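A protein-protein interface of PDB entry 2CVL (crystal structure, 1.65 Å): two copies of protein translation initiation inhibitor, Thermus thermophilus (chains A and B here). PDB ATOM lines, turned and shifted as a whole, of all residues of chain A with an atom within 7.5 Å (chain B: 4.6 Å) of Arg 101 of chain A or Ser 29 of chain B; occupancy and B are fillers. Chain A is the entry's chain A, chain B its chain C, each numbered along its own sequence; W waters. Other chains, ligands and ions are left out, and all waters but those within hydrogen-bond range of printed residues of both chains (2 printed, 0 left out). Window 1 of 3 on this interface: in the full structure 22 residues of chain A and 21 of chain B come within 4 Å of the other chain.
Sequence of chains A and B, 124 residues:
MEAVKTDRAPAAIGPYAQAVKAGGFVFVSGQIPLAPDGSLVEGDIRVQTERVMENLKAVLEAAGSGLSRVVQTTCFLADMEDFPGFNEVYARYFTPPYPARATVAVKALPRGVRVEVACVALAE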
ATOM      1  N   VAL A  71     -23.943   6.095  16.637  1.00  0.00           N
ATOM      2  CA  VAL A  71     -24.243   4.726  16.229  1.00  0.00           C
ATOM      3  C   VAL A  71     -25.652   4.548  15.682  1.00  0.00           C
ATOM      4  O   VAL A  71     -25.946   3.555  15.021  1.00  0.00           O
ATOM      5  CB  VAL A  71     -24.068   3.743  17.414  1.00  0.00           C
ATOM      6  CG1 VAL A  71     -22.641   3.793  17.927  1.00  0.00           C
ATOM      7  CG2 VAL A  71     -25.042   4.098  18.537  1.00  0.00           C
ATOM      8  N   GLN A  72     -26.521   5.516  15.945  1.00  0.00           N
ATOM      9  CA  GLN A  72     -27.900   5.417  15.500  1.00  0.00           C
ATOM     10  C   GLN A  72     -28.539   6.788  15.365  1.00  0.00           C
ATOM     11  O   GLN A  72     -28.332   7.660  16.207  1.00  0.00           O
ATOM     12  CB  GLN A  72     -28.698   4.602  16.526  1.00  0.00           C
ATOM     13  CG  GLN A  72     -30.154   4.375  16.167  1.00  0.00           C
ATOM     14  CD  GLN A  72     -31.020   4.148  17.393  1.00  0.00           C
ATOM     15  OE1 GLN A  72     -31.202   5.050  18.216  1.00  0.00           O
ATOM     16  NE2 GLN A  72     -31.559   2.940  17.521  1.00  0.00           N
ATOM     17  N   THR A  73     -29.306   6.978  14.298  1.00  0.00           N
ATOM     18  CA  THR A  73     -30.025   8.230  14.107  1.00  0.00           C
ATOM     19  C   THR A  73     -31.463   7.886  13.734  1.00  0.00           C
ATOM     20  O   THR A  73     -31.737   6.828  13.151  1.00  0.00           O
ATOM     21  CB  THR A  73     -29.416   9.117  12.983  1.00  0.00           C
ATOM     22  OG1 THR A  73     -29.485   8.429  11.731  1.00  0.00           O
ATOM     23  CG2 THR A  73     -27.971   9.466  13.297  1.00  0.00           C
ATOM     24  N   THR A  74     -32.381   8.764  14.113  1.00  0.00           N
ATOM     25  CA  THR A  74     -33.792   8.600  13.798  1.00  0.00           C
ATOM     26  C   THR A  74     -34.123   9.918  13.120  1.00  0.00           C
ATOM     27  O   THR A  74     -34.033  10.986  13.734  1.00  0.00           O
ATOM     28  CB  THR A  74     -34.637   8.411  15.071  1.00  0.00           C
ATOM     29  OG1 THR A  74     -34.155   7.268  15.792  1.00  0.00           O
ATOM     30  CG2 THR A  74     -36.100   8.188  14.712  1.00  0.00           C
ATOM     31  N   CYS A  75     -34.490   9.833  11.846  1.00  0.00           N
ATOM     32  CA  CYS A  75     -34.758  11.015  11.041  1.00  0.00           C
ATOM     33  C   CYS A  75     -36.198  11.150  10.559  1.00  0.00           C
ATOM     34  O   CYS A  75     -36.808  10.188  10.092  1.00  0.00           O
ATOM     35  CB  CYS A  75     -33.813  11.005   9.838  1.00  0.00           C
ATOM     36  SG  CYS A  75     -32.110  10.558  10.259  1.00  0.00           S
ATOM     37  N   PHE A  83     -35.800  13.805   0.636  1.00  0.00           N
ATOM     38  CA  PHE A  83     -34.840  12.807   1.078  1.00  0.00           C
ATOM     39  C   PHE A  83     -33.502  12.831   0.345  1.00  0.00           C
ATOM     40  O   PHE A  83     -32.453  12.744   0.974  1.00  0.00           O
ATOM     41  CB  PHE A  83     -35.412  11.394   0.992  1.00  0.00           C
ATOM     42  CG  PHE A  83     -34.466  10.349   1.499  1.00  0.00           C
ATOM     43  CD1 PHE A  83     -34.157  10.276   2.855  1.00  0.00           C
ATOM     44  CD2 PHE A  83     -33.829   9.478   0.618  1.00  0.00           C
ATOM     45  CE1 PHE A  83     -33.225   9.354   3.328  1.00  0.00           C
ATOM     46  CE2 PHE A  83     -32.895   8.552   1.080  1.00  0.00           C
ATOM     47  CZ  PHE A  83     -32.592   8.491   2.439  1.00  0.00           C
ATOM     48  N   PHE A  86     -31.532  15.706   1.704  1.00  0.00           N
ATOM     49  CA  PHE A  86     -31.259  15.472   3.113  1.00  0.00           C
ATOM     50  C   PHE A  86     -30.135  14.460   3.234  1.00  0.00           C
ATOM     51  O   PHE A  86     -29.196  14.643   4.010  1.00  0.00           O
ATOM     52  CB  PHE A  86     -32.512  14.945   3.825  1.00  0.00           C
ATOM     53  CG  PHE A  86     -32.220  14.255   5.129  1.00  0.00           C
ATOM     54  CD1 PHE A  86     -32.144  12.866   5.193  1.00  0.00           C
ATOM     55  CD2 PHE A  86     -31.996  14.992   6.286  1.00  0.00           C
ATOM     56  CE1 PHE A  86     -31.848  12.219   6.391  1.00  0.00           C
ATOM     57  CE2 PHE A  86     -31.697  14.357   7.495  1.00  0.00           C
ATOM     58  CZ  PHE A  86     -31.624  12.964   7.545  1.00  0.00           C
ATOM     59  N   ASN A  87     -30.231  13.394   2.447  1.00  0.00           N
ATOM     60  CA  ASN A  87     -29.235  12.340   2.479  1.00  0.00           C
ATOM     61  C   ASN A  87     -27.852  12.837   2.069  1.00  0.00           C
ATOM     62  O   ASN A  87     -26.845  12.422   2.641  1.00  0.00           O
ATOM     63  CB  ASN A  87     -29.672  11.184   1.576  1.00  0.00           C
ATOM     64  CG  ASN A  87     -28.861   9.929   1.809  1.00  0.00           C
ATOM     65  OD1 ASN A  87     -28.733   9.462   2.941  1.00  0.00           O
ATOM     66  ND2 ASN A  87     -28.310   9.372   0.737  1.00  0.00           N
ATOM     67  N   GLU A  88     -27.798  13.735   1.089  1.00  0.00           N
ATOM     68  CA  GLU A  88     -26.515  14.249   0.629  1.00  0.00           C
ATOM     69  C   GLU A  88     -25.798  15.078   1.691  1.00  0.00           C
ATOM     70  O   GLU A  88     -24.596  14.916   1.902  1.00  0.00           O
ATOM     71  CB  GLU A  88     -26.691  15.093  -0.633  1.00  0.00           C
ATOM     72  CG  GLU A  88     -25.404  15.239  -1.424  1.00  0.00           C
ATOM     73  CD  GLU A  88     -25.533  16.202  -2.581  1.00  0.00           C
ATOM     74  OE1 GLU A  88     -26.620  16.249  -3.194  1.00  0.00           O
ATOM     75  OE2 GLU A  88     -24.542  16.904  -2.880  1.00  0.00           O
ATOM     76  N   TYR A  90     -26.455  15.001   4.898  1.00  0.00           N
ATOM     77  CA  TYR A  90     -26.251  14.077   6.005  1.00  0.00           C
ATOM     78  C   TYR A  90     -24.909  13.369   5.786  1.00  0.00           C
ATOM     79  O   TYR A  90     -24.098  13.237   6.709  1.00  0.00           O
ATOM     80  CB  TYR A  90     -27.405  13.066   6.016  1.00  0.00           C
ATOM     81  CG  TYR A  90     -27.378  12.033   7.118  1.00  0.00           C
ATOM     82  CD1 TYR A  90     -28.130  12.202   8.283  1.00  0.00           C
ATOM     83  CD2 TYR A  90     -26.645  10.861   6.973  1.00  0.00           C
ATOM     84  CE1 TYR A  90     -28.151  11.213   9.271  1.00  0.00           C
ATOM     85  CE2 TYR A  90     -26.654   9.876   7.947  1.00  0.00           C
ATOM     86  CZ  TYR A  90     -27.409  10.053   9.092  1.00  0.00           C
ATOM     87  OH  TYR A  90     -27.420   9.052  10.033  1.00  0.00           O
ATOM     88  N   ALA A  91     -24.674  12.940   4.547  1.00  0.00           N
ATOM     89  CA  ALA A  91     -23.448  12.238   4.180  1.00  0.00           C
ATOM     90  C   ALA A  91     -22.191  13.088   4.338  1.00  0.00           C
ATOM     91  O   ALA A  91     -21.087  12.557   4.456  1.00  0.00           O
ATOM     92  CB  ALA A  91     -23.553  11.729   2.740  1.00  0.00           C
ATOM     93  N   PHE A  94     -20.913  12.601   8.074  1.00  0.00           N
ATOM     94  CA  PHE A  94     -20.502  11.279   8.527  1.00  0.00           C
ATOM     95  C   PHE A  94     -19.552  10.599   7.550  1.00  0.00           C
ATOM     96  O   PHE A  94     -19.575  10.863   6.347  1.00  0.00           O
ATOM     97  CB  PHE A  94     -21.725  10.386   8.754  1.00  0.00           C
ATOM     98  CG  PHE A  94     -22.632  10.865   9.850  1.00  0.00           C
ATOM     99  CD1 PHE A  94     -23.869  11.425   9.553  1.00  0.00           C
ATOM    100  CD2 PHE A  94     -22.246  10.766  11.183  1.00  0.00           C
ATOM    101  CE1 PHE A  94     -24.711  11.878  10.563  1.00  0.00           C
ATOM    102  CE2 PHE A  94     -23.081  11.218  12.205  1.00  0.00           C
ATOM    103  CZ  PHE A  94     -24.314  11.774  11.897  1.00  0.00           C
ATOM    104  N   TYR A  98     -20.690   4.385   9.022  1.00  0.00           N
ATOM    105  CA  TYR A  98     -21.854   5.247   9.215  1.00  0.00           C
ATOM    106  C   TYR A  98     -22.800   4.715  10.281  1.00  0.00           C
ATOM    107  O   TYR A  98     -22.795   3.525  10.595  1.00  0.00           O
ATOM    108  CB  TYR A  98     -22.645   5.401   7.913  1.00  0.00           C
ATOM    109  CG  TYR A  98     -21.872   6.003   6.765  1.00  0.00           C
ATOM    110  CD1 TYR A  98     -21.231   5.192   5.830  1.00  0.00           C
ATOM    111  CD2 TYR A  98     -21.787   7.386   6.607  1.00  0.00           C
ATOM    112  CE1 TYR A  98     -20.524   5.744   4.764  1.00  0.00           C
ATOM    113  CE2 TYR A  98     -21.081   7.948   5.546  1.00  0.00           C
ATOM    114  CZ  TYR A  98     -20.453   7.120   4.629  1.00  0.00           C
ATOM    115  OH  TYR A  98     -19.752   7.668   3.579  1.00  0.00           O
ATOM    116  N   PRO A  99     -23.639   5.598  10.846  1.00  0.00           N
ATOM    117  CA  PRO A  99     -24.583   5.164  11.880  1.00  0.00           C
ATOM    118  C   PRO A  99     -25.709   4.317  11.294  1.00  0.00           C
ATOM    119  O   PRO A  99     -25.932   4.311  10.077  1.00  0.00           O
ATOM    120  CB  PRO A  99     -25.135   6.484  12.432  1.00  0.00           C
ATOM    121  CG  PRO A  99     -24.079   7.505  12.082  1.00  0.00           C
ATOM    122  CD  PRO A  99     -23.654   7.064  10.702  1.00  0.00           C
ATOM    123  N   ALA A 100     -26.397   3.583  12.164  1.00  0.00           N
ATOM    124  CA  ALA A 100     -27.554   2.804  11.749  1.00  0.00           C
ATOM    125  C   ALA A 100     -28.591   3.916  11.626  1.00  0.00           C
ATOM    126  O   ALA A 100     -28.499   4.917  12.339  1.00  0.00           O
ATOM    127  CB  ALA A 100     -27.953   1.809  12.840  1.00  0.00           C
ATOM    128  N   ARG A 101     -29.571   3.763  10.741  1.00  0.00           N
ATOM    129  CA  ARG A 101     -30.548   4.830  10.554  1.00  0.00           C
ATOM    130  C   ARG A 101     -31.960   4.363  10.237  1.00  0.00           C
ATOM    131  O   ARG A 101     -32.161   3.325   9.617  1.00  0.00           O
ATOM    132  CB  ARG A 101     -30.063   5.762   9.426  1.00  0.00           C
ATOM    133  CG  ARG A 101     -30.973   6.960   9.132  1.00  0.00           C
ATOM    134  CD  ARG A 101     -30.351   7.940   8.131  1.00  0.00           C
ATOM    135  NE  ARG A 101     -30.268   7.389   6.780  1.00  0.00           N
ATOM    136  CZ  ARG A 101     -29.853   8.071   5.716  1.00  0.00           C
ATOM    137  NH1 ARG A 101     -29.476   9.337   5.839  1.00  0.00           N
ATOM    138  NH2 ARG A 101     -29.814   7.485   4.525  1.00  0.00           N
ATOM    139  N   ALA A 102     -32.933   5.145  10.692  1.00  0.00           N
ATOM    140  CA  ALA A 102     -34.342   4.894  10.419  1.00  0.00           C
ATOM    141  C   ALA A 102     -34.856   6.243   9.944  1.00  0.00           C
ATOM    142  O   ALA A 102     -34.575   7.266  10.565  1.00  0.00           O
ATOM    143  CB  ALA A 102     -35.079   4.460  11.681  1.00  0.00           C
ATOM    144  N   THR A 103     -35.584   6.256   8.832  1.00  0.00           N
ATOM    145  CA  THR A 103     -36.110   7.504   8.291  1.00  0.00           C
ATOM    146  C   THR A 103     -37.575   7.339   7.911  1.00  0.00           C
ATOM    147  O   THR A 103     -37.964   6.317   7.336  1.00  0.00           O
ATOM    148  CB  THR A 103     -35.322   7.942   7.029  1.00  0.00           C
ATOM    149  OG1 THR A 103     -33.939   8.118   7.361  1.00  0.00           O
ATOM    150  CG2 THR A 103     -35.864   9.251   6.484  1.00  0.00           C
ATOM    151  N   VAL A 117     -33.858  15.451  13.420  1.00  0.00           N
ATOM    152  CA  VAL A 117     -33.026  14.274  13.646  1.00  0.00           C
ATOM    153  C   VAL A 117     -32.606  14.122  15.102  1.00  0.00           C
ATOM    154  O   VAL A 117     -32.166  15.079  15.730  1.00  0.00           O
ATOM    155  CB  VAL A 117     -31.732  14.326  12.792  1.00  0.00           C
ATOM    156  CG1 VAL A 117     -30.870  13.104  13.078  1.00  0.00           C
ATOM    157  CG2 VAL A 117     -32.080  14.384  11.311  1.00  0.00           C
ATOM    158  N   PRO B  15     -25.115   7.131   3.263  1.00  0.00           N
ATOM    159  CA  PRO B  15     -24.413   7.334   4.533  1.00  0.00           C
ATOM    160  C   PRO B  15     -25.039   6.612   5.724  1.00  0.00           C
ATOM    161  O   PRO B  15     -25.485   7.246   6.677  1.00  0.00           O
ATOM    162  CB  PRO B  15     -24.446   8.848   4.694  1.00  0.00           C
ATOM    163  CG  PRO B  15     -25.793   9.188   4.133  1.00  0.00           C
ATOM    164  CD  PRO B  15     -25.852   8.345   2.872  1.00  0.00           C
ATOM    165  N   TYR B  16     -25.065   5.285   5.665  1.00  0.00           N
ATOM    166  CA  TYR B  16     -25.619   4.487   6.751  1.00  0.00           C
ATOM    167  C   TYR B  16     -25.144   3.049   6.617  1.00  0.00           C
ATOM    168  O   TYR B  16     -24.746   2.616   5.535  1.00  0.00           O
ATOM    169  CB  TYR B  16     -27.153   4.535   6.721  1.00  0.00           C
ATOM    170  CG  TYR B  16     -27.785   3.699   5.630  1.00  0.00           C
ATOM    171  CD1 TYR B  16     -28.192   2.388   5.878  1.00  0.00           C
ATOM    172  CD2 TYR B  16     -27.963   4.215   4.346  1.00  0.00           C
ATOM    173  CE1 TYR B  16     -28.761   1.606   4.874  1.00  0.00           C
ATOM    174  CE2 TYR B  16     -28.532   3.442   3.333  1.00  0.00           C
ATOM    175  CZ  TYR B  16     -28.928   2.140   3.605  1.00  0.00           C
ATOM    176  OH  TYR B  16     -29.488   1.371   2.609  1.00  0.00           O
ATOM    177  N   ALA B  17     -25.169   2.321   7.726  1.00  0.00           N
ATOM    178  CA  ALA B  17     -24.763   0.922   7.744  1.00  0.00           C
ATOM    179  C   ALA B  17     -25.999   0.096   8.062  1.00  0.00           C
ATOM    180  O   ALA B  17     -26.907   0.580   8.742  1.00  0.00           O
ATOM    181  CB  ALA B  17     -23.693   0.700   8.809  1.00  0.00           C
ATOM    182  N   GLN B  18     -26.040  -1.141   7.576  1.00  0.00           N
ATOM    183  CA  GLN B  18     -27.185  -2.004   7.833  1.00  0.00           C
ATOM    184  C   GLN B  18     -27.357  -2.118   9.340  1.00  0.00           C
ATOM    185  O   GLN B  18     -28.477  -2.152   9.849  1.00  0.00           O
ATOM    186  CB  GLN B  18     -26.955  -3.387   7.218  1.00  0.00           C
ATOM    187  CG  GLN B  18     -26.846  -3.358   5.701  1.00  0.00           C
ATOM    188  CD  GLN B  18     -26.358  -4.671   5.125  1.00  0.00           C
ATOM    189  OE1 GLN B  18     -25.369  -5.231   5.593  1.00  0.00           O
ATOM    190  NE2 GLN B  18     -27.045  -5.164   4.096  1.00  0.00           N
ATOM    191  N   ALA B  19     -26.233  -2.176  10.046  1.00  0.00           N
ATOM    192  CA  ALA B  19     -26.244  -2.256  11.500  1.00  0.00           C
ATOM    193  C   ALA B  19     -24.881  -1.843  12.030  1.00  0.00           C
ATOM    194  O   ALA B  19     -23.891  -1.871  11.302  1.00  0.00           O
ATOM    195  CB  ALA B  19     -26.574  -3.663  11.954  1.00  0.00           C
ATOM    196  N   PHE B  27     -27.157  -2.007  16.761  1.00  0.00           N
ATOM    197  CA  PHE B  27     -28.167  -1.053  16.331  1.00  0.00           C
ATOM    198  C   PHE B  27     -28.440  -1.345  14.861  1.00  0.00           C
ATOM    199  O   PHE B  27     -27.565  -1.179  14.012  1.00  0.00           O
ATOM    200  CB  PHE B  27     -27.649   0.377  16.518  1.00  0.00           C
ATOM    201  CG  PHE B  27     -27.381   0.736  17.956  1.00  0.00           C
ATOM    202  CD1 PHE B  27     -28.362   1.354  18.727  1.00  0.00           C
ATOM    203  CD2 PHE B  27     -26.165   0.417  18.553  1.00  0.00           C
ATOM    204  CE1 PHE B  27     -28.139   1.644  20.068  1.00  0.00           C
ATOM    205  CE2 PHE B  27     -25.933   0.703  19.897  1.00  0.00           C
ATOM    206  CZ  PHE B  27     -26.920   1.316  20.654  1.00  0.00           C
ATOM    207  N   VAL B  28     -29.660  -1.791  14.573  1.00  0.00           N
ATOM    208  CA  VAL B  28     -30.050  -2.145  13.216  1.00  0.00           C
ATOM    209  C   VAL B  28     -30.873  -1.052  12.548  1.00  0.00           C
ATOM    210  O   VAL B  28     -31.843  -0.549  13.123  1.00  0.00           O
ATOM    211  CB  VAL B  28     -30.862  -3.464  13.223  1.00  0.00           C
ATOM    212  CG1 VAL B  28     -31.188  -3.892  11.804  1.00  0.00           C
ATOM    213  CG2 VAL B  28     -30.062  -4.565  13.929  1.00  0.00           C
ATOM    214  N   SER B  29     -30.474  -0.681  11.334  1.00  0.00           N
ATOM    215  CA  SER B  29     -31.182   0.350  10.582  1.00  0.00           C
ATOM    216  C   SER B  29     -32.606  -0.097  10.274  1.00  0.00           C
ATOM    217  O   SER B  29     -32.914  -1.288  10.303  1.00  0.00           O
ATOM    218  CB  SER B  29     -30.456   0.649   9.261  1.00  0.00           C
ATOM    219  OG  SER B  29     -29.218   1.295   9.496  1.00  0.00           O
ATOM    220  N   GLY B  30     -33.471   0.866   9.980  1.00  0.00           N
ATOM    221  CA  GLY B  30     -34.844   0.530   9.648  1.00  0.00           C
ATOM    222  C   GLY B  30     -34.902  -0.282   8.367  1.00  0.00           C
ATOM    223  O   GLY B  30     -34.508   0.191   7.297  1.00  0.00           O
ATOM    224  N   GLN B  31     -35.382  -1.513   8.479  1.00  0.00           N
ATOM    225  CA  GLN B  31     -35.498  -2.393   7.323  1.00  0.00           C
ATOM    226  C   GLN B  31     -36.847  -2.223   6.645  1.00  0.00           C
ATOM    227  O   GLN B  31     -37.872  -2.049   7.313  1.00  0.00           O
ATOM    228  CB  GLN B  31     -35.323  -3.851   7.749  1.00  0.00           C
ATOM    229  CG  GLN B  31     -33.990  -4.122   8.426  1.00  0.00           C
ATOM    230  CD  GLN B  31     -32.810  -3.715   7.563  1.00  0.00           C
ATOM    231  OE1 GLN B  31     -31.936  -2.960   7.999  1.00  0.00           O
ATOM    232  NE2 GLN B  31     -32.776  -4.210   6.332  1.00  0.00           N
ATOM    233  N   VAL B 117     -39.075  -1.377   9.976  1.00  0.00           N
ATOM    234  CA  VAL B 117     -38.766  -1.776  11.344  1.00  0.00           C
ATOM    235  C   VAL B 117     -37.280  -1.682  11.643  1.00  0.00           C
ATOM    236  O   VAL B 117     -36.463  -2.252  10.930  1.00  0.00           O
ATOM    237  CB  VAL B 117     -39.205  -3.236  11.636  1.00  0.00           C
ATOM    238  CG1 VAL B 117     -38.823  -3.618  13.069  1.00  0.00           C
ATOM    239  CG2 VAL B 117     -40.701  -3.388  11.438  1.00  0.00           C
ATOM    240  N   ALA B 118     -36.943  -0.955  12.705  1.00  0.00           N
ATOM    241  CA  ALA B 118     -35.556  -0.821  13.142  1.00  0.00           C
ATOM    242  C   ALA B 118     -35.506  -1.513  14.496  1.00  0.00           C
ATOM    243  O   ALA B 118     -36.545  -1.741  15.103  1.00  0.00           O
ATOM    244  CB  ALA B 118     -35.180   0.652  13.286  1.00  0.00           C
HETATM  245  O   HOH W   1     -26.625   6.845   8.967  1.00  0.00           O
HETATM  246  O   HOH W   2     -31.640   1.184  15.194  1.00  0.00           O
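The side-chain hydroxyl (OG) of Ser 29 of chain B sits at hydrogen-bond distance from the backbone NH (N) of Arg 101 of chain A, 2.8 Å away. O of Arg 101 of chain A lies within hydrogen-bond range of N of Gly 30 of chain B. The backbone NH (N) of Ala 17 of chain B sits at hydrogen-bond distance from the backbone carbonyl oxygen (O) of Pro 99 of chain A (3.2 Å).
The backbone carbonyl oxygen of Ala 100 of chain A is in hydrogen-bond range of the backbone NH of Thr 73 of chain A (3.0 Å). OG1 of Thr 73 of chain A is in hydrogen-bond range of OH of Tyr 90 of chain A (2.7 Å). OD1 of Asn 87 of chain A lies within hydrogen-bond range of NH2 of Arg 101 of chain A (2.8 Å). N of Ala 100 of chain A sits at hydrogen-bond distance from O of Val 71 of chain A (2.9 Å). O of Gln 18 of chain B is in hydrogen-bond range of N of Ser 29 of chain B (2.9 Å). The backbone carbonyl oxygen (O) of Ser 29 of chain B sits close to the side-chain amide oxygen (OE1) of Gln 31 of chain B (3.0 Å).
Phe 27 of chain B touches Val 71 of chain A. Phe 27 of chain B touches Gln 72 of chain A (CD1 to NE2, 3.8 Å). Asn 87 of chain A touches Pro 15 of chain B. Tyr 90 of chain A touches Pro 15 of chain B. CD2 of Tyr 98 of chain A touches CA of Pro 15 of chain B, 3.3 Å away. Tyr 98 of chain A touches Tyr 16 of chain B. Ala 100 of chain A touches Ala 17 of chain B. Phe 27 of chain B touches Ala 100 of chain A. Ser 29 of chain B touches Ala 100 of chain A. Arg 101 of chain A touches Tyr 16 of chain B (NH2 to CD2, 3.8 Å).
Printed residues of chain B within 4 Å of Tyr 98 of chain A: Pro 15, Tyr 16 and Ala 17. Arg 101 of chain A touches just these residues of chain B: Tyr 16, Ser 29 and Gly 30. Of the printed residues of chain A, Tyr 16 of chain B touches Tyr 98, Pro 99 and Arg 101. Printed residues of chain A within 4 Å of Phe 27 of chain B: Val 71 (3.8 Å), Gln 72 (3.8 Å) and Ala 100 (3.2 Å). Ser 29 of chain B touches just these residues of chain A: Ala 100 and Arg 101. Gln 31 of chain B touches none of the printed residues of chain A. Ala 118 of chain B touches none of the printed residues of chain A. The nearest residue of chain B that does not touch Arg 101 of chain A is Pro 15 of chain B (4.1 Å). The nearest residue of chain A that does not touch Ser 29 of chain B is Pro 99 of chain A (4.5 Å).
Hydrophobic or aromatic side chains of chain A that line the printed part of chain B: Val 71, Tyr 90, Ala 91, Tyr 98 and Ala 100. Hydrophobic or aromatic side chains of chain B within 4 Å of the printed part of chain A: Pro 15, Tyr 16, Ala 17 and Phe 27. Among the printed residues, 16 pairs touch across the chains. Among the printed residues, no Asp or Glu carboxylate lies within 4 Å of a Lys or Arg side-chain nitrogen of the other chain.
Position printed for both chains: 117.
Water W1 lies within hydrogen-bond range of the side-chain hydroxyl of Tyr 90 of chain A, the backbone carbonyl oxygen of Pro 15 of chain B and the backbone carbonyl oxygen of Pro 99 of chain A. Water W2 lies within hydrogen-bond range of the backbone carbonyl oxygen (O) of Val 28 of chain B (2.7 Å) and the side-chain amide nitrogen (NE2) of Gln 72 of chain A (2.9 Å).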
